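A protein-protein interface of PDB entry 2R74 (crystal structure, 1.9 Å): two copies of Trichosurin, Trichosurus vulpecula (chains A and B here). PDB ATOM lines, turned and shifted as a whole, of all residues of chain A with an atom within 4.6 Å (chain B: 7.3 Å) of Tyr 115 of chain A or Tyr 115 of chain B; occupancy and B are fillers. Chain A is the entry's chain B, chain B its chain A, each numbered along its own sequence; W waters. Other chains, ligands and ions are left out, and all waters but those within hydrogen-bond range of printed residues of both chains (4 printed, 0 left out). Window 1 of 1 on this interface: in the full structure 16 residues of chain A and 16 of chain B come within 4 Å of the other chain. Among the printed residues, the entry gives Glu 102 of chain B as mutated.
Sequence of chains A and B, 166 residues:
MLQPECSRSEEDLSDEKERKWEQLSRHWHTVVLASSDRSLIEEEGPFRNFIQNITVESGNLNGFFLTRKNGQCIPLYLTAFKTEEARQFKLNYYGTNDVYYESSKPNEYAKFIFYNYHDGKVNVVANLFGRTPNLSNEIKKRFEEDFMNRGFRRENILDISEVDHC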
ATOM      1  N   THR A  96      23.425   8.836  26.237  1.00  0.00           N
ATOM      2  CA  THR A  96      24.123  10.063  26.600  1.00  0.00           C
ATOM      3  C   THR A  96      23.179  11.252  26.432  1.00  0.00           C
ATOM      4  O   THR A  96      22.184  11.162  25.715  1.00  0.00           O
ATOM      5  CB  THR A  96      25.401  10.258  25.738  1.00  0.00           C
ATOM      6  OG1 THR A  96      25.074  10.157  24.344  1.00  0.00           O
ATOM      7  CG2 THR A  96      26.433   9.190  26.079  1.00  0.00           C
ATOM      8  N   ASN A  97      23.474  12.361  27.104  1.00  0.00           N
ATOM      9  CA  ASN A  97      22.606  13.532  26.999  1.00  0.00           C
ATOM     10  C   ASN A  97      23.337  14.854  27.081  1.00  0.00           C
ATOM     11  O   ASN A  97      24.253  15.017  27.885  1.00  0.00           O
ATOM     12  CB  ASN A  97      21.561  13.571  28.122  1.00  0.00           C
ATOM     13  CG  ASN A  97      20.884  12.244  28.359  1.00  0.00           C
ATOM     14  OD1 ASN A  97      21.452  11.347  28.989  1.00  0.00           O
ATOM     15  ND2 ASN A  97      19.653  12.111  27.869  1.00  0.00           N
ATOM     16  N   ASP A  98      22.932  15.796  26.239  1.00  0.00           N
ATOM     17  CA  ASP A  98      23.474  17.138  26.323  1.00  0.00           C
ATOM     18  C   ASP A  98      22.323  17.807  27.073  1.00  0.00           C
ATOM     19  O   ASP A  98      21.165  17.716  26.651  1.00  0.00           O
ATOM     20  CB  ASP A  98      23.682  17.748  24.936  1.00  0.00           C
ATOM     21  CG  ASP A  98      24.975  17.274  24.291  1.00  0.00           C
ATOM     22  OD1 ASP A  98      26.044  17.453  24.919  1.00  0.00           O
ATOM     23  OD2 ASP A  98      24.931  16.725  23.167  1.00  0.00           O
ATOM     24  N   TYR A 100      20.604  21.275  28.971  1.00  0.00           N
ATOM     25  CA  TYR A 100      20.604  22.734  29.034  1.00  0.00           C
ATOM     26  C   TYR A 100      19.650  23.257  30.097  1.00  0.00           C
ATOM     27  O   TYR A 100      18.499  22.810  30.195  1.00  0.00           O
ATOM     28  CB  TYR A 100      20.221  23.353  27.686  1.00  0.00           C
ATOM     29  CG  TYR A 100      21.216  23.093  26.587  1.00  0.00           C
ATOM     30  CD1 TYR A 100      21.181  21.909  25.858  1.00  0.00           C
ATOM     31  CD2 TYR A 100      22.203  24.026  26.285  1.00  0.00           C
ATOM     32  CE1 TYR A 100      22.098  21.660  24.853  1.00  0.00           C
ATOM     33  CE2 TYR A 100      23.129  23.787  25.283  1.00  0.00           C
ATOM     34  CZ  TYR A 100      23.068  22.600  24.570  1.00  0.00           C
ATOM     35  OH  TYR A 100      23.979  22.353  23.571  1.00  0.00           O
ATOM     36  N   ILE A 113      16.415  20.983  29.663  1.00  0.00           N
ATOM     37  CA  ILE A 113      16.145  20.328  28.396  1.00  0.00           C
ATOM     38  C   ILE A 113      17.192  19.242  28.206  1.00  0.00           C
ATOM     39  O   ILE A 113      18.397  19.507  28.252  1.00  0.00           O
ATOM     40  CB  ILE A 113      16.259  21.299  27.212  1.00  0.00           C
ATOM     41  CG1 ILE A 113      15.303  22.482  27.398  1.00  0.00           C
ATOM     42  CG2 ILE A 113      15.959  20.550  25.908  1.00  0.00           C
ATOM     43  CD1 ILE A 113      13.840  22.085  27.493  1.00  0.00           C
ATOM     44  N   PHE A 114      16.735  18.014  28.011  1.00  0.00           N
ATOM     45  CA  PHE A 114      17.645  16.911  27.792  1.00  0.00           C
ATOM     46  C   PHE A 114      17.568  16.463  26.340  1.00  0.00           C
ATOM     47  O   PHE A 114      16.501  16.062  25.863  1.00  0.00           O
ATOM     48  CB  PHE A 114      17.291  15.712  28.687  1.00  0.00           C
ATOM     49  CG  PHE A 114      17.473  15.964  30.161  1.00  0.00           C
ATOM     50  CD1 PHE A 114      16.567  16.744  30.867  1.00  0.00           C
ATOM     51  CD2 PHE A 114      18.549  15.416  30.840  1.00  0.00           C
ATOM     52  CE1 PHE A 114      16.734  16.968  32.226  1.00  0.00           C
ATOM     53  CE2 PHE A 114      18.722  15.640  32.199  1.00  0.00           C
ATOM     54  CZ  PHE A 114      17.815  16.415  32.891  1.00  0.00           C
ATOM     55  N   TYR A 115      18.685  16.560  25.630  1.00  0.00           N
ATOM     56  CA  TYR A 115      18.736  16.067  24.263  1.00  0.00           C
ATOM     57  C   TYR A 115      19.378  14.705  24.474  1.00  0.00           C
ATOM     58  O   TYR A 115      20.587  14.591  24.711  1.00  0.00           O
ATOM     59  CB  TYR A 115      19.601  16.966  23.384  1.00  0.00           C
ATOM     60  CG  TYR A 115      18.945  18.300  23.106  1.00  0.00           C
ATOM     61  CD1 TYR A 115      17.834  18.389  22.273  1.00  0.00           C
ATOM     62  CD2 TYR A 115      19.414  19.463  23.696  1.00  0.00           C
ATOM     63  CE1 TYR A 115      17.210  19.608  22.037  1.00  0.00           C
ATOM     64  CE2 TYR A 115      18.799  20.682  23.468  1.00  0.00           C
ATOM     65  CZ  TYR A 115      17.700  20.747  22.638  1.00  0.00           C
ATOM     66  OH  TYR A 115      17.091  21.960  22.417  1.00  0.00           O
ATOM     67  N   ASN A 116      18.537  13.680  24.432  1.00  0.00           N
ATOM     68  CA  ASN A 116      18.955  12.307  24.662  1.00  0.00           C
ATOM     69  C   ASN A 116      19.345  11.560  23.394  1.00  0.00           C
ATOM     70  O   ASN A 116      18.649  11.633  22.384  1.00  0.00           O
ATOM     71  CB  ASN A 116      17.822  11.557  25.366  1.00  0.00           C
ATOM     72  CG  ASN A 116      18.163  10.110  25.642  1.00  0.00           C
ATOM     73  OD1 ASN A 116      19.003   9.807  26.495  1.00  0.00           O
ATOM     74  ND2 ASN A 116      17.514   9.204  24.917  1.00  0.00           N
ATOM     75  N   TYR A 117      20.462  10.843  23.458  1.00  0.00           N
ATOM     76  CA  TYR A 117      20.944  10.053  22.330  1.00  0.00           C
ATOM     77  C   TYR A 117      20.920   8.596  22.803  1.00  0.00           C
ATOM     78  O   TYR A 117      21.729   8.195  23.635  1.00  0.00           O
ATOM     79  CB  TYR A 117      22.375  10.468  21.957  1.00  0.00           C
ATOM     80  CG  TYR A 117      22.571  11.969  21.842  1.00  0.00           C
ATOM     81  CD1 TYR A 117      21.922  12.705  20.856  1.00  0.00           C
ATOM     82  CD2 TYR A 117      23.376  12.655  22.745  1.00  0.00           C
ATOM     83  CE1 TYR A 117      22.067  14.087  20.775  1.00  0.00           C
ATOM     84  CE2 TYR A 117      23.527  14.031  22.675  1.00  0.00           C
ATOM     85  CZ  TYR A 117      22.868  14.742  21.690  1.00  0.00           C
ATOM     86  OH  TYR A 117      22.999  16.110  21.637  1.00  0.00           O
ATOM     87  N   ASN A 123      16.027  12.232  20.981  1.00  0.00           N
ATOM     88  CA  ASN A 123      14.740  12.633  21.552  1.00  0.00           C
ATOM     89  C   ASN A 123      14.970  13.826  22.468  1.00  0.00           C
ATOM     90  O   ASN A 123      16.059  13.990  23.016  1.00  0.00           O
ATOM     91  CB  ASN A 123      14.095  11.500  22.359  1.00  0.00           C
ATOM     92  CG  ASN A 123      13.359  10.491  21.480  1.00  0.00           C
ATOM     93  OD1 ASN A 123      13.745   9.327  21.412  1.00  0.00           O
ATOM     94  ND2 ASN A 123      12.296  10.940  20.804  1.00  0.00           N
ATOM     95  N   VAL A 124      13.956  14.667  22.621  1.00  0.00           N
ATOM     96  CA  VAL A 124      14.077  15.818  23.499  1.00  0.00           C
ATOM     97  C   VAL A 124      13.134  15.623  24.672  1.00  0.00           C
ATOM     98  O   VAL A 124      11.967  15.277  24.491  1.00  0.00           O
ATOM     99  CB  VAL A 124      13.734  17.146  22.773  1.00  0.00           C
ATOM    100  CG1 VAL A 124      12.350  17.073  22.157  1.00  0.00           C
ATOM    101  CG2 VAL A 124      13.814  18.311  23.760  1.00  0.00           C
ATOM    102  N   PHE B  47      20.114  19.269   4.773  1.00  0.00           N
ATOM    103  CA  PHE B  47      21.152  19.928   5.564  1.00  0.00           C
ATOM    104  C   PHE B  47      22.539  19.891   4.938  1.00  0.00           C
ATOM    105  O   PHE B  47      23.533  20.209   5.602  1.00  0.00           O
ATOM    106  CB  PHE B  47      21.206  19.351   6.984  1.00  0.00           C
ATOM    107  CG  PHE B  47      20.097  19.840   7.869  1.00  0.00           C
ATOM    108  CD1 PHE B  47      18.846  19.244   7.837  1.00  0.00           C
ATOM    109  CD2 PHE B  47      20.295  20.925   8.707  1.00  0.00           C
ATOM    110  CE1 PHE B  47      17.813  19.723   8.624  1.00  0.00           C
ATOM    111  CE2 PHE B  47      19.264  21.410   9.496  1.00  0.00           C
ATOM    112  CZ  PHE B  47      18.022  20.808   9.456  1.00  0.00           C
ATOM    113  N   GLN B  88      22.318  30.655  21.722  1.00  0.00           N
ATOM    114  CA  GLN B  88      21.207  29.783  21.358  1.00  0.00           C
ATOM    115  C   GLN B  88      20.323  30.552  20.385  1.00  0.00           C
ATOM    116  O   GLN B  88      19.979  31.714  20.629  1.00  0.00           O
ATOM    117  CB  GLN B  88      20.371  29.363  22.567  1.00  0.00           C
ATOM    118  CG  GLN B  88      19.171  28.501  22.147  1.00  0.00           C
ATOM    119  CD  GLN B  88      18.394  27.925  23.314  1.00  0.00           C
ATOM    120  OE1 GLN B  88      17.355  27.288  23.127  1.00  0.00           O
ATOM    121  NE2 GLN B  88      18.892  28.142  24.523  1.00  0.00           N
ATOM    122  N   LEU B  91      15.646  28.756  14.335  1.00  0.00           N
ATOM    123  CA  LEU B  91      15.635  28.815  12.881  1.00  0.00           C
ATOM    124  C   LEU B  91      14.489  28.015  12.290  1.00  0.00           C
ATOM    125  O   LEU B  91      14.237  26.887  12.701  1.00  0.00           O
ATOM    126  CB  LEU B  91      16.948  28.278  12.309  1.00  0.00           C
ATOM    127  CG  LEU B  91      16.884  28.026  10.799  1.00  0.00           C
ATOM    128  CD1 LEU B  91      16.791  29.362  10.082  1.00  0.00           C
ATOM    129  CD2 LEU B  91      18.102  27.248  10.329  1.00  0.00           C
ATOM    130  N   THR B  96      11.326  23.093  12.321  1.00  0.00           N
ATOM    131  CA  THR B  96      11.841  24.076  13.266  1.00  0.00           C
ATOM    132  C   THR B  96      13.169  23.571  13.829  1.00  0.00           C
ATOM    133  O   THR B  96      13.421  22.371  13.841  1.00  0.00           O
ATOM    134  CB  THR B  96      10.831  24.328  14.403  1.00  0.00           C
ATOM    135  OG1 THR B  96      11.301  25.399  15.225  1.00  0.00           O
ATOM    136  CG2 THR B  96      10.657  23.089  15.249  1.00  0.00           C
ATOM    137  N   ASN B  97      14.024  24.479  14.287  1.00  0.00           N
ATOM    138  CA  ASN B  97      15.326  24.067  14.811  1.00  0.00           C
ATOM    139  C   ASN B  97      15.795  24.885  16.000  1.00  0.00           C
ATOM    140  O   ASN B  97      15.625  26.105  16.031  1.00  0.00           O
ATOM    141  CB  ASN B  97      16.413  24.208  13.734  1.00  0.00           C
ATOM    142  CG  ASN B  97      16.055  23.525  12.430  1.00  0.00           C
ATOM    143  OD1 ASN B  97      16.406  22.363  12.199  1.00  0.00           O
ATOM    144  ND2 ASN B  97      15.353  24.250  11.560  1.00  0.00           N
ATOM    145  N   ASP B  98      16.385  24.202  16.975  1.00  0.00           N
ATOM    146  CA  ASP B  98      16.982  24.865  18.125  1.00  0.00           C
ATOM    147  C   ASP B  98      18.452  24.868  17.696  1.00  0.00           C
ATOM    148  O   ASP B  98      19.006  23.810  17.406  1.00  0.00           O
ATOM    149  CB  ASP B  98      16.830  24.032  19.400  1.00  0.00           C
ATOM    150  CG  ASP B  98      15.414  24.021  19.931  1.00  0.00           C
ATOM    151  OD1 ASP B  98      14.772  25.090  19.931  1.00  0.00           O
ATOM    152  OD2 ASP B  98      14.954  22.946  20.375  1.00  0.00           O
ATOM    153  N   VAL B  99      19.075  26.039  17.645  1.00  0.00           N
ATOM    154  CA  VAL B  99      20.466  26.147  17.209  1.00  0.00           C
ATOM    155  C   VAL B  99      21.411  26.619  18.314  1.00  0.00           C
ATOM    156  O   VAL B  99      21.184  27.662  18.928  1.00  0.00           O
ATOM    157  CB  VAL B  99      20.585  27.130  16.017  1.00  0.00           C
ATOM    158  CG1 VAL B  99      22.029  27.191  15.526  1.00  0.00           C
ATOM    159  CG2 VAL B  99      19.648  26.705  14.892  1.00  0.00           C
ATOM    160  N   TYR B 100      22.477  25.855  18.550  1.00  0.00           N
ATOM    161  CA  TYR B 100      23.458  26.198  19.573  1.00  0.00           C
ATOM    162  C   TYR B 100      24.833  26.422  18.959  1.00  0.00           C
ATOM    163  O   TYR B 100      25.321  25.600  18.181  1.00  0.00           O
ATOM    164  CB  TYR B 100      23.543  25.084  20.624  1.00  0.00           C
ATOM    165  CG  TYR B 100      22.266  24.905  21.419  1.00  0.00           C
ATOM    166  CD1 TYR B 100      22.041  25.619  22.591  1.00  0.00           C
ATOM    167  CD2 TYR B 100      21.279  24.028  20.987  1.00  0.00           C
ATOM    168  CE1 TYR B 100      20.867  25.458  23.309  1.00  0.00           C
ATOM    169  CE2 TYR B 100      20.108  23.864  21.691  1.00  0.00           C
ATOM    170  CZ  TYR B 100      19.905  24.573  22.847  1.00  0.00           C
ATOM    171  OH  TYR B 100      18.735  24.389  23.544  1.00  0.00           O
ATOM    172  N   GLU B 102      28.957  27.052  19.457  1.00  0.00           N
ATOM    173  CA  GLU B 102      30.049  26.727  20.366  1.00  0.00           C
ATOM    174  C   GLU B 102      31.390  26.951  19.661  1.00  0.00           C
ATOM    175  O   GLU B 102      31.490  26.801  18.447  1.00  0.00           O
ATOM    176  CB  GLU B 102      29.990  25.254  20.805  1.00  0.00           C
ATOM    177  CG  GLU B 102      28.695  24.789  21.422  1.00  0.00           C
ATOM    178  CD  GLU B 102      28.755  23.348  21.904  1.00  0.00           C
ATOM    179  OE1 GLU B 102      29.623  22.596  21.434  1.00  0.00           O
ATOM    180  OE2 GLU B 102      27.921  22.970  22.738  1.00  0.00           O
ATOM    181  N   ILE B 113      25.275  23.421  16.339  1.00  0.00           N
ATOM    182  CA  ILE B 113      24.526  22.188  16.536  1.00  0.00           C
ATOM    183  C   ILE B 113      23.051  22.464  16.274  1.00  0.00           C
ATOM    184  O   ILE B 113      22.446  23.301  16.939  1.00  0.00           O
ATOM    185  CB  ILE B 113      24.662  21.685  17.975  1.00  0.00           C
ATOM    186  CG1 ILE B 113      26.131  21.410  18.288  1.00  0.00           C
ATOM    187  CG2 ILE B 113      23.806  20.438  18.169  1.00  0.00           C
ATOM    188  CD1 ILE B 113      26.388  21.127  19.756  1.00  0.00           C
ATOM    189  N   PHE B 114      22.480  21.762  15.303  1.00  0.00           N
ATOM    190  CA  PHE B 114      21.076  21.937  14.978  1.00  0.00           C
ATOM    191  C   PHE B 114      20.257  20.754  15.457  1.00  0.00           C
ATOM    192  O   PHE B 114      20.568  19.600  15.143  1.00  0.00           O
ATOM    193  CB  PHE B 114      20.857  22.046  13.464  1.00  0.00           C
ATOM    194  CG  PHE B 114      21.354  23.321  12.853  1.00  0.00           C
ATOM    195  CD1 PHE B 114      22.706  23.613  12.819  1.00  0.00           C
ATOM    196  CD2 PHE B 114      20.465  24.219  12.283  1.00  0.00           C
ATOM    197  CE1 PHE B 114      23.162  24.781  12.224  1.00  0.00           C
ATOM    198  CE2 PHE B 114      20.916  25.384  11.690  1.00  0.00           C
ATOM    199  CZ  PHE B 114      22.264  25.664  11.662  1.00  0.00           C
ATOM    200  N   TYR B 115      19.214  21.044  16.219  1.00  0.00           N
ATOM    201  CA  TYR B 115      18.295  20.009  16.664  1.00  0.00           C
ATOM    202  C   TYR B 115      17.073  20.296  15.803  1.00  0.00           C
ATOM    203  O   TYR B 115      16.343  21.259  16.045  1.00  0.00           O
ATOM    204  CB  TYR B 115      17.968  20.159  18.149  1.00  0.00           C
ATOM    205  CG  TYR B 115      19.123  19.766  19.044  1.00  0.00           C
ATOM    206  CD1 TYR B 115      19.941  20.729  19.623  1.00  0.00           C
ATOM    207  CD2 TYR B 115      19.418  18.430  19.272  1.00  0.00           C
ATOM    208  CE1 TYR B 115      21.024  20.368  20.403  1.00  0.00           C
ATOM    209  CE2 TYR B 115      20.500  18.058  20.047  1.00  0.00           C
ATOM    210  CZ  TYR B 115      21.299  19.032  20.609  1.00  0.00           C
ATOM    211  OH  TYR B 115      22.387  18.665  21.363  1.00  0.00           O
ATOM    212  N   ASN B 116      16.882  19.476  14.777  1.00  0.00           N
ATOM    213  CA  ASN B 116      15.778  19.656  13.844  1.00  0.00           C
ATOM    214  C   ASN B 116      14.529  18.874  14.217  1.00  0.00           C
ATOM    215  O   ASN B 116      14.596  17.684  14.517  1.00  0.00           O
ATOM    216  CB  ASN B 116      16.235  19.271  12.433  1.00  0.00           C
ATOM    217  CG  ASN B 116      15.100  19.281  11.425  1.00  0.00           C
ATOM    218  OD1 ASN B 116      14.539  18.236  11.094  1.00  0.00           O
ATOM    219  ND2 ASN B 116      14.756  20.464  10.931  1.00  0.00           N
ATOM    220  N   TYR B 117      13.395  19.564  14.211  1.00  0.00           N
ATOM    221  CA  TYR B 117      12.116  18.940  14.522  1.00  0.00           C
ATOM    222  C   TYR B 117      11.317  18.900  13.234  1.00  0.00           C
ATOM    223  O   TYR B 117      10.751  19.907  12.816  1.00  0.00           O
ATOM    224  CB  TYR B 117      11.356  19.750  15.569  1.00  0.00           C
ATOM    225  CG  TYR B 117      12.130  19.971  16.844  1.00  0.00           C
ATOM    226  CD1 TYR B 117      12.939  21.089  17.004  1.00  0.00           C
ATOM    227  CD2 TYR B 117      12.071  19.049  17.879  1.00  0.00           C
ATOM    228  CE1 TYR B 117      13.669  21.283  18.164  1.00  0.00           C
ATOM    229  CE2 TYR B 117      12.797  19.232  19.040  1.00  0.00           C
ATOM    230  CZ  TYR B 117      13.592  20.351  19.176  1.00  0.00           C
ATOM    231  OH  TYR B 117      14.309  20.534  20.332  1.00  0.00           O
ATOM    232  N   HIS B 118      11.295  17.733  12.602  1.00  0.00           N
ATOM    233  CA  HIS B 118      10.578  17.559  11.350  1.00  0.00           C
ATOM    234  C   HIS B 118       9.398  16.624  11.579  1.00  0.00           C
ATOM    235  O   HIS B 118       9.571  15.421  11.786  1.00  0.00           O
ATOM    236  CB  HIS B 118      11.509  16.974  10.285  1.00  0.00           C
ATOM    237  CG  HIS B 118      10.936  17.003   8.903  1.00  0.00           C
ATOM    238  ND1 HIS B 118      10.746  18.174   8.201  1.00  0.00           N
ATOM    239  CD2 HIS B 118      10.492  16.008   8.099  1.00  0.00           C
ATOM    240  CE1 HIS B 118      10.211  17.899   7.025  1.00  0.00           C
ATOM    241  NE2 HIS B 118      10.047  16.591   6.939  1.00  0.00           N
ATOM    242  N   LYS B 121       9.573  14.311  14.495  1.00  0.00           N
ATOM    243  CA  LYS B 121      10.816  13.574  14.690  1.00  0.00           C
ATOM    244  C   LYS B 121      12.014  14.490  14.897  1.00  0.00           C
ATOM    245  O   LYS B 121      12.168  15.506  14.216  1.00  0.00           O
ATOM    246  CB  LYS B 121      11.111  12.627  13.525  1.00  0.00           C
ATOM    247  CG  LYS B 121      12.380  11.815  13.780  1.00  0.00           C
ATOM    248  CD  LYS B 121      12.626  10.735  12.749  1.00  0.00           C
ATOM    249  CE  LYS B 121      13.831   9.890  13.146  1.00  0.00           C
ATOM    250  NZ  LYS B 121      14.108   8.807  12.161  1.00  0.00           N
ATOM    251  N   VAL B 122      12.872  14.101  15.833  1.00  0.00           N
ATOM    252  CA  VAL B 122      14.051  14.881  16.169  1.00  0.00           C
ATOM    253  C   VAL B 122      15.332  14.276  15.600  1.00  0.00           C
ATOM    254  O   VAL B 122      15.528  13.059  15.613  1.00  0.00           O
ATOM    255  CB  VAL B 122      14.209  14.993  17.707  1.00  0.00           C
ATOM    256  CG1 VAL B 122      15.320  15.979  18.055  1.00  0.00           C
ATOM    257  CG2 VAL B 122      12.894  15.423  18.334  1.00  0.00           C
ATOM    258  N   ASN B 123      16.196  15.143  15.085  1.00  0.00           N
ATOM    259  CA  ASN B 123      17.487  14.733  14.553  1.00  0.00           C
ATOM    260  C   ASN B 123      18.488  15.805  14.965  1.00  0.00           C
ATOM    261  O   ASN B 123      18.115  16.949  15.221  1.00  0.00           O
ATOM    262  CB  ASN B 123      17.467  14.625  13.019  1.00  0.00           C
ATOM    263  CG  ASN B 123      16.919  13.289  12.525  1.00  0.00           C
ATOM    264  OD1 ASN B 123      15.836  13.227  11.939  1.00  0.00           O
ATOM    265  ND2 ASN B 123      17.671  12.216  12.758  1.00  0.00           N
ATOM    266  N   VAL B 124      19.753  15.426  15.049  1.00  0.00           N
ATOM    267  CA  VAL B 124      20.791  16.379  15.396  1.00  0.00           C
ATOM    268  C   VAL B 124      21.716  16.481  14.193  1.00  0.00           C
ATOM    269  O   VAL B 124      22.083  15.476  13.596  1.00  0.00           O
ATOM    270  CB  VAL B 124      21.592  15.923  16.640  1.00  0.00           C
ATOM    271  CG1 VAL B 124      22.208  14.556  16.396  1.00  0.00           C
ATOM    272  CG2 VAL B 124      22.683  16.947  16.968  1.00  0.00           C
ATOM    273  N   VAL B 125      22.055  17.707  13.813  1.00  0.00           N
ATOM    274  CA  VAL B 125      22.960  17.940  12.695  1.00  0.00           C
ATOM    275  C   VAL B 125      24.038  18.884  13.216  1.00  0.00           C
ATOM    276  O   VAL B 125      23.754  20.036  13.548  1.00  0.00           O
ATOM    277  CB  VAL B 125      22.244  18.611  11.501  1.00  0.00           C
ATOM    278  CG1 VAL B 125      23.231  18.812  10.356  1.00  0.00           C
ATOM    279  CG2 VAL B 125      21.072  17.747  11.032  1.00  0.00           C
ATOM    280  N   ALA B 126      25.268  18.390  13.291  1.00  0.00           N
ATOM    281  CA  ALA B 126      26.384  19.189  13.786  1.00  0.00           C
ATOM    282  C   ALA B 126      27.200  19.716  12.619  1.00  0.00           C
ATOM    283  O   ALA B 126      27.559  18.961  11.713  1.00  0.00           O
ATOM    284  CB  ALA B 126      27.273  18.342  14.709  1.00  0.00           C
ATOM    285  N   ARG B 150      28.507   9.998  21.364  1.00  0.00           N
ATOM    286  CA  ARG B 150      27.073  10.106  21.603  1.00  0.00           C
ATOM    287  C   ARG B 150      26.295   8.984  20.907  1.00  0.00           C
ATOM    288  O   ARG B 150      25.096   9.104  20.636  1.00  0.00           O
ATOM    289  CB  ARG B 150      26.586  11.493  21.169  1.00  0.00           C
ATOM    290  CG  ARG B 150      27.115  12.610  22.081  1.00  0.00           C
ATOM    291  CD  ARG B 150      26.818  14.012  21.554  1.00  0.00           C
ATOM    292  NE  ARG B 150      27.102  15.051  22.549  1.00  0.00           N
ATOM    293  CZ  ARG B 150      28.308  15.326  23.044  1.00  0.00           C
ATOM    294  NH1 ARG B 150      29.374  14.645  22.641  1.00  0.00           N
ATOM    295  NH2 ARG B 150      28.448  16.276  23.960  1.00  0.00           N
HETATM  296  O   HOH W   1      24.198  20.305  22.187  1.00  0.00           O
HETATM  297  O   HOH W   2      22.947   6.904  20.702  1.00  0.00           O
HETATM  298  O   HOH W   3      25.847  24.311  23.136  1.00  0.00           O
HETATM  299  O   HOH W   4      24.994   7.219  23.573  1.00  0.00           O
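The side-chain carboxylate (OD2) of Asp 98 of chain B is in hydrogen-bond range of the side-chain hydroxyl (OH) of Tyr 115 of chain A (3.1 Å).
The side-chain hydroxyl (OH) of Tyr 100 of chain B is in hydrogen-bond range of the side-chain hydroxyl (OH) of Tyr 115 of chain A, 3.1 Å away.
The side-chain hydroxyl (OH) of Tyr 115 of chain B sits at hydrogen-bond distance from the side-chain hydroxyl (OH) of Tyr 117 of chain A.
The side-chain carboxylate of Asp 98 of chain A lies within salt-bridge range of the guanidinium group of Arg 150 of chain B (2.8 Å).
O of Tyr 100 of chain B sits at hydrogen-bond distance from N of Ile 113 of chain B, 2.9 Å away.
O of Thr 96 of chain A sits at hydrogen-bond distance from N of Tyr 117 of chain A.
The side-chain carboxylate of Asp 98 of chain A lies within hydrogen-bond range of the side-chain hydroxyl of Tyr 117 of chain A (2.5 Å).
Among the printed residues, merely in contact across the chains: Tyr 117 of chain A with Arg 150 of chain B (3.3 Å), Thr 96 of chain A with Arg 150 of chain B (3.4 Å), Tyr 115 of chain A with Tyr 115 of chain B (3.4 Å), Tyr 100 of chain A with Tyr 100 of chain B (3.4 Å), Tyr 115 of chain A with Tyr 117 of chain B (3.5 Å), Asp 98 of chain A with Tyr 115 of chain B (3.7 Å) and Val 124 of chain A with Tyr 117 of chain B (3.8 Å).
Of the printed residues of chain B, Thr 96 of chain A touches Arg 150 (3.4 Å).
Tyr 115 of chain A touches just these residues of chain B: Asp 98 (3.1 Å), Tyr 100 (3.1 Å), Tyr 115 (3.4 Å) and Tyr 117 (3.5 Å).
Of the printed residues of chain B, Tyr 117 of chain A touches Tyr 115 (2.6 Å) and Arg 150 (3.3 Å).
Of chain A, only Asp 98 (3.7 Å), Tyr 115 (3.4 Å) and Tyr 117 (2.6 Å) come within 4 Å of Tyr 115 of chain B.
The nearest residue of chain B that does not touch Tyr 115 of chain A is Gln 88 of chain B (5.4 Å).
The nearest printed residue of chain A that does not touch Tyr 115 of chain B is Tyr 100 of chain A (4.6 Å).
The nearest printed residue of chain B that does not touch Tyr 117 of chain A is Val 124 of chain B (4.4 Å).
Printed residues of chain A that touch a printed residue of chain B: Thr 96, Asp 98, Tyr 100, Tyr 115, Tyr 117 and Val 124.
Hydrophobic or aromatic side chains of chain A that line the printed part of chain B: Tyr 100, Tyr 115, Tyr 117 and Val 124.
Of the 22 printed residues of chain B, 5 touch a printed residue of chain A.
Among the printed residues, 11 pairs touch across the chains.
Among the printed residues, Asp or Glu carboxylates within 4 Å of a Lys or Arg side-chain nitrogen of the other chain: Asp 98 of chain A with Arg 150 of chain B.
Tyr 100 of chain A touches its own counterpart, Tyr 100 of chain B.
Tyr 115 of chain A touches Tyr 100 of chain B, but with the chains exchanged Tyr 100 of chain A does not touch Tyr 115 of chain B (4.6 Å).
Val 124 of chain A touches Tyr 117 of chain B, but with the chains exchanged Tyr 117 of chain A does not touch Val 124 of chain B (4.4 Å).
Water W1 lies within hydrogen-bond range of OH of Tyr 100 of chain A (2.5 Å) and OH of Tyr 115 of chain B (2.6 Å).
Water W3 lies within hydrogen-bond range of the side-chain carboxylate of Glu 102 of chain B and the side-chain hydroxyl of Tyr 100 of chain A.
Water W2 bridges the backbone carbonyl oxygen (O) of Arg 150 of chain B (3.1 Å) and the backbone carbonyl oxygen (O) of Tyr 117 of chain A (3.4 Å).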
